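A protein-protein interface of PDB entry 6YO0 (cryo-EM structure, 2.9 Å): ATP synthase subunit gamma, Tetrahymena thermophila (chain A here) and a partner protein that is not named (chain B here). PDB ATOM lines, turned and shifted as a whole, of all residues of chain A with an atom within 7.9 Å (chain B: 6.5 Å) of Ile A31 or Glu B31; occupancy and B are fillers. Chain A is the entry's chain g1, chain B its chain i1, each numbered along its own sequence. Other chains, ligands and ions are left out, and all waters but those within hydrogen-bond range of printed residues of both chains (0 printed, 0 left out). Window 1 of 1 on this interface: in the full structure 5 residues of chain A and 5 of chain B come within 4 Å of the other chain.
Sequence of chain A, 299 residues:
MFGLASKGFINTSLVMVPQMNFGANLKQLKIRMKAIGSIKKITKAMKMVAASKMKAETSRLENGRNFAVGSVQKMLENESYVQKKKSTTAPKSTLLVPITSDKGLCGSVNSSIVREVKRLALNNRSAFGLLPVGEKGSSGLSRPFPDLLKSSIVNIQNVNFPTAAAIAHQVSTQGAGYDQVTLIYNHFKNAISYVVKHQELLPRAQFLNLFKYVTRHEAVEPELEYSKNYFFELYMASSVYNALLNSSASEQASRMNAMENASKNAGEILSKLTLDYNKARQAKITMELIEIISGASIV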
ATOM      1  N   ASN A  25      -6.591 -30.724  38.342  1.00  0.00           N
ATOM      2  CA  ASN A  25      -5.604 -29.671  38.565  1.00  0.00           C
ATOM      3  C   ASN A  25      -5.839 -28.510  37.593  1.00  0.00           C
ATOM      4  O   ASN A  25      -5.040 -28.225  36.700  1.00  0.00           O
ATOM      5  CB  ASN A  25      -4.179 -30.216  38.444  1.00  0.00           C
ATOM      6  CG  ASN A  25      -3.144 -29.247  38.981  1.00  0.00           C
ATOM      7  OD1 ASN A  25      -3.383 -28.041  39.047  1.00  0.00           O
ATOM      8  ND2 ASN A  25      -1.989 -29.771  39.372  1.00  0.00           N
ATOM      9  N   LEU A  26      -6.981 -27.857  37.799  1.00  0.00           N
ATOM     10  CA  LEU A  26      -7.456 -26.785  36.931  1.00  0.00           C
ATOM     11  C   LEU A  26      -6.337 -25.848  36.512  1.00  0.00           C
ATOM     12  O   LEU A  26      -6.387 -25.258  35.429  1.00  0.00           O
ATOM     13  CB  LEU A  26      -8.529 -25.956  37.634  1.00  0.00           C
ATOM     14  CG  LEU A  26      -9.853 -26.575  38.057  1.00  0.00           C
ATOM     15  CD1 LEU A  26      -9.698 -27.535  39.215  1.00  0.00           C
ATOM     16  CD2 LEU A  26     -10.756 -25.436  38.425  1.00  0.00           C
ATOM     17  N   LYS A  27      -5.322 -25.706  37.360  1.00  0.00           N
ATOM     18  CA  LYS A  27      -4.206 -24.836  37.019  1.00  0.00           C
ATOM     19  C   LYS A  27      -3.508 -25.343  35.766  1.00  0.00           C
ATOM     20  O   LYS A  27      -3.200 -24.569  34.854  1.00  0.00           O
ATOM     21  CB  LYS A  27      -3.237 -24.768  38.193  1.00  0.00           C
ATOM     22  CG  LYS A  27      -2.322 -23.571  38.172  1.00  0.00           C
ATOM     23  CD  LYS A  27      -1.531 -23.474  39.464  1.00  0.00           C
ATOM     24  CE  LYS A  27      -0.605 -22.268  39.468  1.00  0.00           C
ATOM     25  NZ  LYS A  27       0.416 -22.339  38.395  1.00  0.00           N
ATOM     26  N   GLN A  28      -3.262 -26.650  35.700  1.00  0.00           N
ATOM     27  CA  GLN A  28      -2.642 -27.227  34.516  1.00  0.00           C
ATOM     28  C   GLN A  28      -3.553 -27.106  33.303  1.00  0.00           C
ATOM     29  O   GLN A  28      -3.092 -26.786  32.201  1.00  0.00           O
ATOM     30  CB  GLN A  28      -2.291 -28.691  34.771  1.00  0.00           C
ATOM     31  CG  GLN A  28      -1.430 -28.918  35.993  1.00  0.00           C
ATOM     32  CD  GLN A  28      -0.079 -28.235  35.920  1.00  0.00           C
ATOM     33  OE1 GLN A  28       0.195 -27.457  35.009  1.00  0.00           O
ATOM     34  NE2 GLN A  28       0.769 -28.511  36.901  1.00  0.00           N
ATOM     35  N   LEU A  29      -4.849 -27.357  33.485  1.00  0.00           N
ATOM     36  CA  LEU A  29      -5.788 -27.226  32.378  1.00  0.00           C
ATOM     37  C   LEU A  29      -5.796 -25.812  31.823  1.00  0.00           C
ATOM     38  O   LEU A  29      -5.804 -25.617  30.603  1.00  0.00           O
ATOM     39  CB  LEU A  29      -7.190 -27.611  32.834  1.00  0.00           C
ATOM     40  CG  LEU A  29      -7.490 -29.097  32.979  1.00  0.00           C
ATOM     41  CD1 LEU A  29      -8.900 -29.281  33.468  1.00  0.00           C
ATOM     42  CD2 LEU A  29      -7.301 -29.799  31.663  1.00  0.00           C
ATOM     43  N   LYS A  30      -5.775 -24.812  32.698  1.00  0.00           N
ATOM     44  CA  LYS A  30      -5.805 -23.436  32.224  1.00  0.00           C
ATOM     45  C   LYS A  30      -4.528 -23.099  31.473  1.00  0.00           C
ATOM     46  O   LYS A  30      -4.560 -22.379  30.469  1.00  0.00           O
ATOM     47  CB  LYS A  30      -6.022 -22.492  33.400  1.00  0.00           C
ATOM     48  CG  LYS A  30      -6.197 -21.042  33.005  1.00  0.00           C
ATOM     49  CD  LYS A  30      -7.078 -20.282  33.985  1.00  0.00           C
ATOM     50  CE  LYS A  30      -6.671 -20.515  35.434  1.00  0.00           C
ATOM     51  NZ  LYS A  30      -7.611 -19.864  36.382  1.00  0.00           N
ATOM     52  N   ILE A  31      -3.395 -23.616  31.942  1.00  0.00           N
ATOM     53  CA  ILE A  31      -2.136 -23.419  31.234  1.00  0.00           C
ATOM     54  C   ILE A  31      -2.218 -24.036  29.846  1.00  0.00           C
ATOM     55  O   ILE A  31      -1.827 -23.423  28.846  1.00  0.00           O
ATOM     56  CB  ILE A  31      -0.975 -24.007  32.052  1.00  0.00           C
ATOM     57  CG1 ILE A  31      -0.786 -23.192  33.330  1.00  0.00           C
ATOM     58  CG2 ILE A  31       0.288 -24.041  31.232  1.00  0.00           C
ATOM     59  CD1 ILE A  31       0.351 -23.649  34.193  1.00  0.00           C
ATOM     60  N   ARG A  32      -2.728 -25.263  29.766  1.00  0.00           N
ATOM     61  CA  ARG A  32      -2.844 -25.928  28.476  1.00  0.00           C
ATOM     62  C   ARG A  32      -3.841 -25.207  27.583  1.00  0.00           C
ATOM     63  O   ARG A  32      -3.650 -25.123  26.365  1.00  0.00           O
ATOM     64  CB  ARG A  32      -3.244 -27.385  28.691  1.00  0.00           C
ATOM     65  CG  ARG A  32      -3.170 -28.240  27.465  1.00  0.00           C
ATOM     66  CD  ARG A  32      -2.811 -29.664  27.807  1.00  0.00           C
ATOM     67  NE  ARG A  32      -3.915 -30.442  28.351  1.00  0.00           N
ATOM     68  CZ  ARG A  32      -4.704 -31.235  27.634  1.00  0.00           C
ATOM     69  NH1 ARG A  32      -4.522 -31.367  26.326  1.00  0.00           N
ATOM     70  NH2 ARG A  32      -5.675 -31.911  28.231  1.00  0.00           N
ATOM     71  N   MET A  33      -4.914 -24.684  28.173  1.00  0.00           N
ATOM     72  CA  MET A  33      -5.873 -23.892  27.416  1.00  0.00           C
ATOM     73  C   MET A  33      -5.226 -22.627  26.871  1.00  0.00           C
ATOM     74  O   MET A  33      -5.446 -22.250  25.715  1.00  0.00           O
ATOM     75  CB  MET A  33      -7.058 -23.550  28.316  1.00  0.00           C
ATOM     76  CG  MET A  33      -7.943 -24.732  28.659  1.00  0.00           C
ATOM     77  SD  MET A  33      -9.158 -24.365  29.937  1.00  0.00           S
ATOM     78  CE  MET A  33      -9.914 -22.891  29.281  1.00  0.00           C
ATOM     79  N   LYS A  34      -4.421 -21.960  27.696  1.00  0.00           N
ATOM     80  CA  LYS A  34      -3.719 -20.757  27.267  1.00  0.00           C
ATOM     81  C   LYS A  34      -2.744 -21.038  26.133  1.00  0.00           C
ATOM     82  O   LYS A  34      -2.634 -20.250  25.188  1.00  0.00           O
ATOM     83  CB  LYS A  34      -2.983 -20.156  28.459  1.00  0.00           C
ATOM     84  CG  LYS A  34      -2.124 -18.964  28.137  1.00  0.00           C
ATOM     85  CD  LYS A  34      -1.375 -18.508  29.367  1.00  0.00           C
ATOM     86  CE  LYS A  34      -0.525 -17.290  29.080  1.00  0.00           C
ATOM     87  NZ  LYS A  34       0.250 -16.874  30.275  1.00  0.00           N
ATOM     88  N   ALA A  35      -2.018 -22.151  26.216  1.00  0.00           N
ATOM     89  CA  ALA A  35      -1.074 -22.504  25.163  1.00  0.00           C
ATOM     90  C   ALA A  35      -1.776 -22.708  23.831  1.00  0.00           C
ATOM     91  O   ALA A  35      -1.340 -22.189  22.798  1.00  0.00           O
ATOM     92  CB  ALA A  35      -0.307 -23.760  25.554  1.00  0.00           C
ATOM     93  N   ILE A  36      -2.875 -23.458  23.836  1.00  0.00           N
ATOM     94  CA  ILE A  36      -3.586 -23.737  22.597  1.00  0.00           C
ATOM     95  C   ILE A  36      -4.158 -22.463  22.004  1.00  0.00           C
ATOM     96  O   ILE A  36      -4.226 -22.317  20.779  1.00  0.00           O
ATOM     97  CB  ILE A  36      -4.682 -24.783  22.854  1.00  0.00           C
ATOM     98  CG1 ILE A  36      -4.037 -26.105  23.254  1.00  0.00           C
ATOM     99  CG2 ILE A  36      -5.532 -24.961  21.623  1.00  0.00           C
ATOM    100  CD1 ILE A  36      -4.997 -27.232  23.392  1.00  0.00           C
ATOM    101  N   GLY A  37      -4.579 -21.525  22.845  1.00  0.00           N
ATOM    102  CA  GLY A  37      -5.075 -20.269  22.321  1.00  0.00           C
ATOM    103  C   GLY A  37      -3.999 -19.485  21.601  1.00  0.00           C
ATOM    104  O   GLY A  37      -4.233 -18.937  20.522  1.00  0.00           O
ATOM    105  N   SER A  38      -2.802 -19.425  22.184  1.00  0.00           N
ATOM    106  CA  SER A  38      -1.691 -18.771  21.505  1.00  0.00           C
ATOM    107  C   SER A  38      -1.361 -19.478  20.199  1.00  0.00           C
ATOM    108  O   SER A  38      -1.129 -18.829  19.173  1.00  0.00           O
ATOM    109  CB  SER A  38      -0.472 -18.741  22.421  1.00  0.00           C
ATOM    110  OG  SER A  38      -0.008 -20.050  22.670  1.00  0.00           O
ATOM    111  N   ILE A  39      -1.358 -20.809  20.212  1.00  0.00           N
ATOM    112  CA  ILE A  39      -1.084 -21.563  18.993  1.00  0.00           C
ATOM    113  C   ILE A  39      -2.132 -21.246  17.939  1.00  0.00           C
ATOM    114  O   ILE A  39      -1.817 -20.995  16.770  1.00  0.00           O
ATOM    115  CB  ILE A  39      -1.033 -23.068  19.298  1.00  0.00           C
ATOM    116  CG1 ILE A  39       0.214 -23.383  20.119  1.00  0.00           C
ATOM    117  CG2 ILE A  39      -1.067 -23.865  18.013  1.00  0.00           C
ATOM    118  CD1 ILE A  39       0.389 -24.834  20.444  1.00  0.00           C
ATOM    119  N   LEU A 273     -11.372 -28.904  25.829  1.00  0.00           N
ATOM    120  CA  LEU A 273     -10.678 -28.667  27.090  1.00  0.00           C
ATOM    121  C   LEU A 273     -11.454 -27.721  27.990  1.00  0.00           C
ATOM    122  O   LEU A 273     -11.394 -27.842  29.217  1.00  0.00           O
ATOM    123  CB  LEU A 273      -9.286 -28.110  26.827  1.00  0.00           C
ATOM    124  CG  LEU A 273      -8.273 -29.053  26.194  1.00  0.00           C
ATOM    125  CD1 LEU A 273      -6.935 -28.399  26.194  1.00  0.00           C
ATOM    126  CD2 LEU A 273      -8.208 -30.353  26.940  1.00  0.00           C
ATOM    127  N   TYR A 277     -12.535 -28.227  31.840  1.00  0.00           N
ATOM    128  CA  TYR A 277     -12.181 -27.264  32.874  1.00  0.00           C
ATOM    129  C   TYR A 277     -13.400 -26.862  33.686  1.00  0.00           C
ATOM    130  O   TYR A 277     -13.324 -26.744  34.914  1.00  0.00           O
ATOM    131  CB  TYR A 277     -11.538 -26.031  32.247  1.00  0.00           C
ATOM    132  CG  TYR A 277     -11.351 -24.891  33.214  1.00  0.00           C
ATOM    133  CD1 TYR A 277     -10.241 -24.827  34.035  1.00  0.00           C
ATOM    134  CD2 TYR A 277     -12.285 -23.876  33.303  1.00  0.00           C
ATOM    135  CE1 TYR A 277     -10.071 -23.788  34.919  1.00  0.00           C
ATOM    136  CE2 TYR A 277     -12.123 -22.836  34.183  1.00  0.00           C
ATOM    137  CZ  TYR A 277     -11.015 -22.797  34.990  1.00  0.00           C
ATOM    138  OH  TYR A 277     -10.850 -21.756  35.871  1.00  0.00           O
ATOM    139  N   ARG B  29       0.932 -31.974  27.267  1.00  0.00           N
ATOM    140  CA  ARG B  29       1.581 -30.742  27.711  1.00  0.00           C
ATOM    141  C   ARG B  29       2.083 -30.000  26.475  1.00  0.00           C
ATOM    142  O   ARG B  29       3.156 -30.312  25.951  1.00  0.00           O
ATOM    143  CB  ARG B  29       2.713 -31.026  28.686  1.00  0.00           C
ATOM    144  CG  ARG B  29       2.267 -31.515  30.055  1.00  0.00           C
ATOM    145  CD  ARG B  29       1.312 -30.548  30.730  1.00  0.00           C
ATOM    146  NE  ARG B  29       1.884 -29.214  30.881  1.00  0.00           N
ATOM    147  CZ  ARG B  29       2.592 -28.813  31.933  1.00  0.00           C
ATOM    148  NH1 ARG B  29       2.830 -29.642  32.942  1.00  0.00           N
ATOM    149  NH2 ARG B  29       3.066 -27.576  31.974  1.00  0.00           N
ATOM    150  N   GLU B  30       1.298 -29.026  26.022  1.00  0.00           N
ATOM    151  CA  GLU B  30       1.666 -28.187  24.892  1.00  0.00           C
ATOM    152  C   GLU B  30       2.484 -26.987  25.332  1.00  0.00           C
ATOM    153  O   GLU B  30       3.280 -26.462  24.547  1.00  0.00           O
ATOM    154  CB  GLU B  30       0.421 -27.704  24.146  1.00  0.00           C
ATOM    155  CG  GLU B  30      -0.401 -28.792  23.468  1.00  0.00           C
ATOM    156  CD  GLU B  30      -0.994 -29.795  24.433  1.00  0.00           C
ATOM    157  OE1 GLU B  30      -0.645 -29.748  25.630  1.00  0.00           O
ATOM    158  OE2 GLU B  30      -1.819 -30.624  23.998  1.00  0.00           O
ATOM    159  N   GLU B  31       2.302 -26.551  26.578  1.00  0.00           N
ATOM    160  CA  GLU B  31       3.057 -25.417  27.093  1.00  0.00           C
ATOM    161  C   GLU B  31       4.533 -25.761  27.201  1.00  0.00           C
ATOM    162  O   GLU B  31       5.395 -24.924  26.914  1.00  0.00           O
ATOM    163  CB  GLU B  31       2.505 -24.998  28.452  1.00  0.00           C
ATOM    164  CG  GLU B  31       3.183 -23.783  29.056  1.00  0.00           C
ATOM    165  CD  GLU B  31       3.116 -22.558  28.170  1.00  0.00           C
ATOM    166  OE1 GLU B  31       2.291 -22.541  27.233  1.00  0.00           O
ATOM    167  OE2 GLU B  31       3.891 -21.609  28.411  1.00  0.00           O
ATOM    168  N   GLU B  32       4.842 -26.983  27.626  1.00  0.00           N
ATOM    169  CA  GLU B  32       6.235 -27.397  27.713  1.00  0.00           C
ATOM    170  C   GLU B  32       6.852 -27.490  26.325  1.00  0.00           C
ATOM    171  O   GLU B  32       8.032 -27.174  26.139  1.00  0.00           O
ATOM    172  CB  GLU B  32       6.334 -28.738  28.434  1.00  0.00           C
ATOM    173  CG  GLU B  32       5.699 -28.759  29.825  1.00  0.00           C
ATOM    174  CD  GLU B  32       6.295 -27.735  30.772  1.00  0.00           C
ATOM    175  OE1 GLU B  32       7.318 -27.112  30.420  1.00  0.00           O
ATOM    176  OE2 GLU B  32       5.734 -27.554  31.873  1.00  0.00           O
ATOM    177  N   TRP B  33       6.066 -27.921  25.339  1.00  0.00           N
ATOM    178  CA  TRP B  33       6.561 -28.002  23.970  1.00  0.00           C
ATOM    179  C   TRP B  33       6.964 -26.629  23.450  1.00  0.00           C
ATOM    180  O   TRP B  33       8.050 -26.458  22.885  1.00  0.00           O
ATOM    181  CB  TRP B  33       5.487 -28.621  23.082  1.00  0.00           C
ATOM    182  CG  TRP B  33       5.860 -28.738  21.649  1.00  0.00           C
ATOM    183  CD1 TRP B  33       6.631 -29.702  21.080  1.00  0.00           C
ATOM    184  CD2 TRP B  33       5.460 -27.866  20.590  1.00  0.00           C
ATOM    185  NE1 TRP B  33       6.742 -29.484  19.731  1.00  0.00           N
ATOM    186  CE2 TRP B  33       6.030 -28.361  19.406  1.00  0.00           C
ATOM    187  CE3 TRP B  33       4.676 -26.713  20.529  1.00  0.00           C
ATOM    188  CZ2 TRP B  33       5.844 -27.742  18.177  1.00  0.00           C
ATOM    189  CZ3 TRP B  33       4.492 -26.103  19.306  1.00  0.00           C
ATOM    190  CH2 TRP B  33       5.074 -26.617  18.148  1.00  0.00           C
ATOM    191  N   LEU B  34       6.099 -25.633  23.637  1.00  0.00           N
ATOM    192  CA  LEU B  34       6.432 -24.275  23.221  1.00  0.00           C
ATOM    193  C   LEU B  34       7.649 -23.752  23.965  1.00  0.00           C
ATOM    194  O   LEU B  34       8.518 -23.100  23.373  1.00  0.00           O
ATOM    195  CB  LEU B  34       5.243 -23.351  23.441  1.00  0.00           C
ATOM    196  CG  LEU B  34       4.036 -23.524  22.526  1.00  0.00           C
ATOM    197  CD1 LEU B  34       2.986 -22.516  22.891  1.00  0.00           C
ATOM    198  CD2 LEU B  34       4.422 -23.347  21.085  1.00  0.00           C
ATOM    199  N   ASP B  35       7.726 -24.015  25.268  1.00  0.00           N
ATOM    200  CA  ASP B  35       8.852 -23.527  26.052  1.00  0.00           C
ATOM    201  C   ASP B  35      10.161 -24.132  25.565  1.00  0.00           C
ATOM    202  O   ASP B  35      11.164 -23.427  25.421  1.00  0.00           O
ATOM    203  CB  ASP B  35       8.621 -23.840  27.527  1.00  0.00           C
ATOM    204  CG  ASP B  35       9.588 -23.123  28.435  1.00  0.00           C
ATOM    205  OD1 ASP B  35       9.470 -21.889  28.581  1.00  0.00           O
ATOM    206  OD2 ASP B  35      10.455 -23.800  29.025  1.00  0.00           O
ATOM    207  N   LYS B  36      10.169 -25.438  25.304  1.00  0.00           N
ATOM    208  CA  LYS B  36      11.373 -26.070  24.784  1.00  0.00           C
ATOM    209  C   LYS B  36      11.723 -25.523  23.408  1.00  0.00           C
ATOM    210  O   LYS B  36      12.890 -25.229  23.125  1.00  0.00           O
ATOM    211  CB  LYS B  36      11.189 -27.582  24.740  1.00  0.00           C
ATOM    212  CG  LYS B  36      11.046 -28.213  26.107  1.00  0.00           C
ATOM    213  CD  LYS B  36      10.895 -29.716  26.013  1.00  0.00           C
ATOM    214  CE  LYS B  36      10.720 -30.342  27.387  1.00  0.00           C
ATOM    215  NZ  LYS B  36      11.864 -30.062  28.289  1.00  0.00           N
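The side-chain carboxylate of Glu B30 is in salt-bridge range of the guanidinium group of Arg A32, at 3.6 Å.
OG of Ser A38 sits at hydrogen-bond distance from O of Ala A35 (2.5 Å). The guanidinium group (NH2) of Arg B29 lies within salt-bridge range of the side-chain carboxylate (OE2) of Glu B32.
Gln A28 touches Arg B29. Glu B31 touches Ile A31 (CG to CG2, 3.6 Å). CB of Ala A35 touches OE1 of Glu B31, at 3.3 Å. Ser A38 touches Leu B34 (OG to CD1, 3.9 Å).
Of chain B, only Glu B31 comes within 4 Å of Ile A31. Printed residues of chain B within 4 Å of Arg A32: Glu B30 (3.1 Å). Of the printed residues of chain B, Ser A38 touches Leu B34 (3.9 Å). Glu B31 touches just these residues of chain A: Ile A31 (3.6 Å) and Ala A35 (3.3 Å). The nearest residue of chain B that does not touch Ile A31 is Arg B29 (4.6 Å). The nearest printed residue of chain B that does not touch Ser A38 is Glu B31 (5.7 Å).
Printed residues of chain A that touch a printed residue of chain B: Gln A28, Ile A31, Arg A32, Ala A35 and Ser A38. Hydrophobic or aromatic side chains of chain B that line the printed part of chain A: Leu B34. Among the printed residues, 5 pairs touch across the chains. Among the printed residues, Asp or Glu carboxylates within 4 Å of a Lys or Arg side-chain nitrogen of the other chain: Arg A32 with Glu B30.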
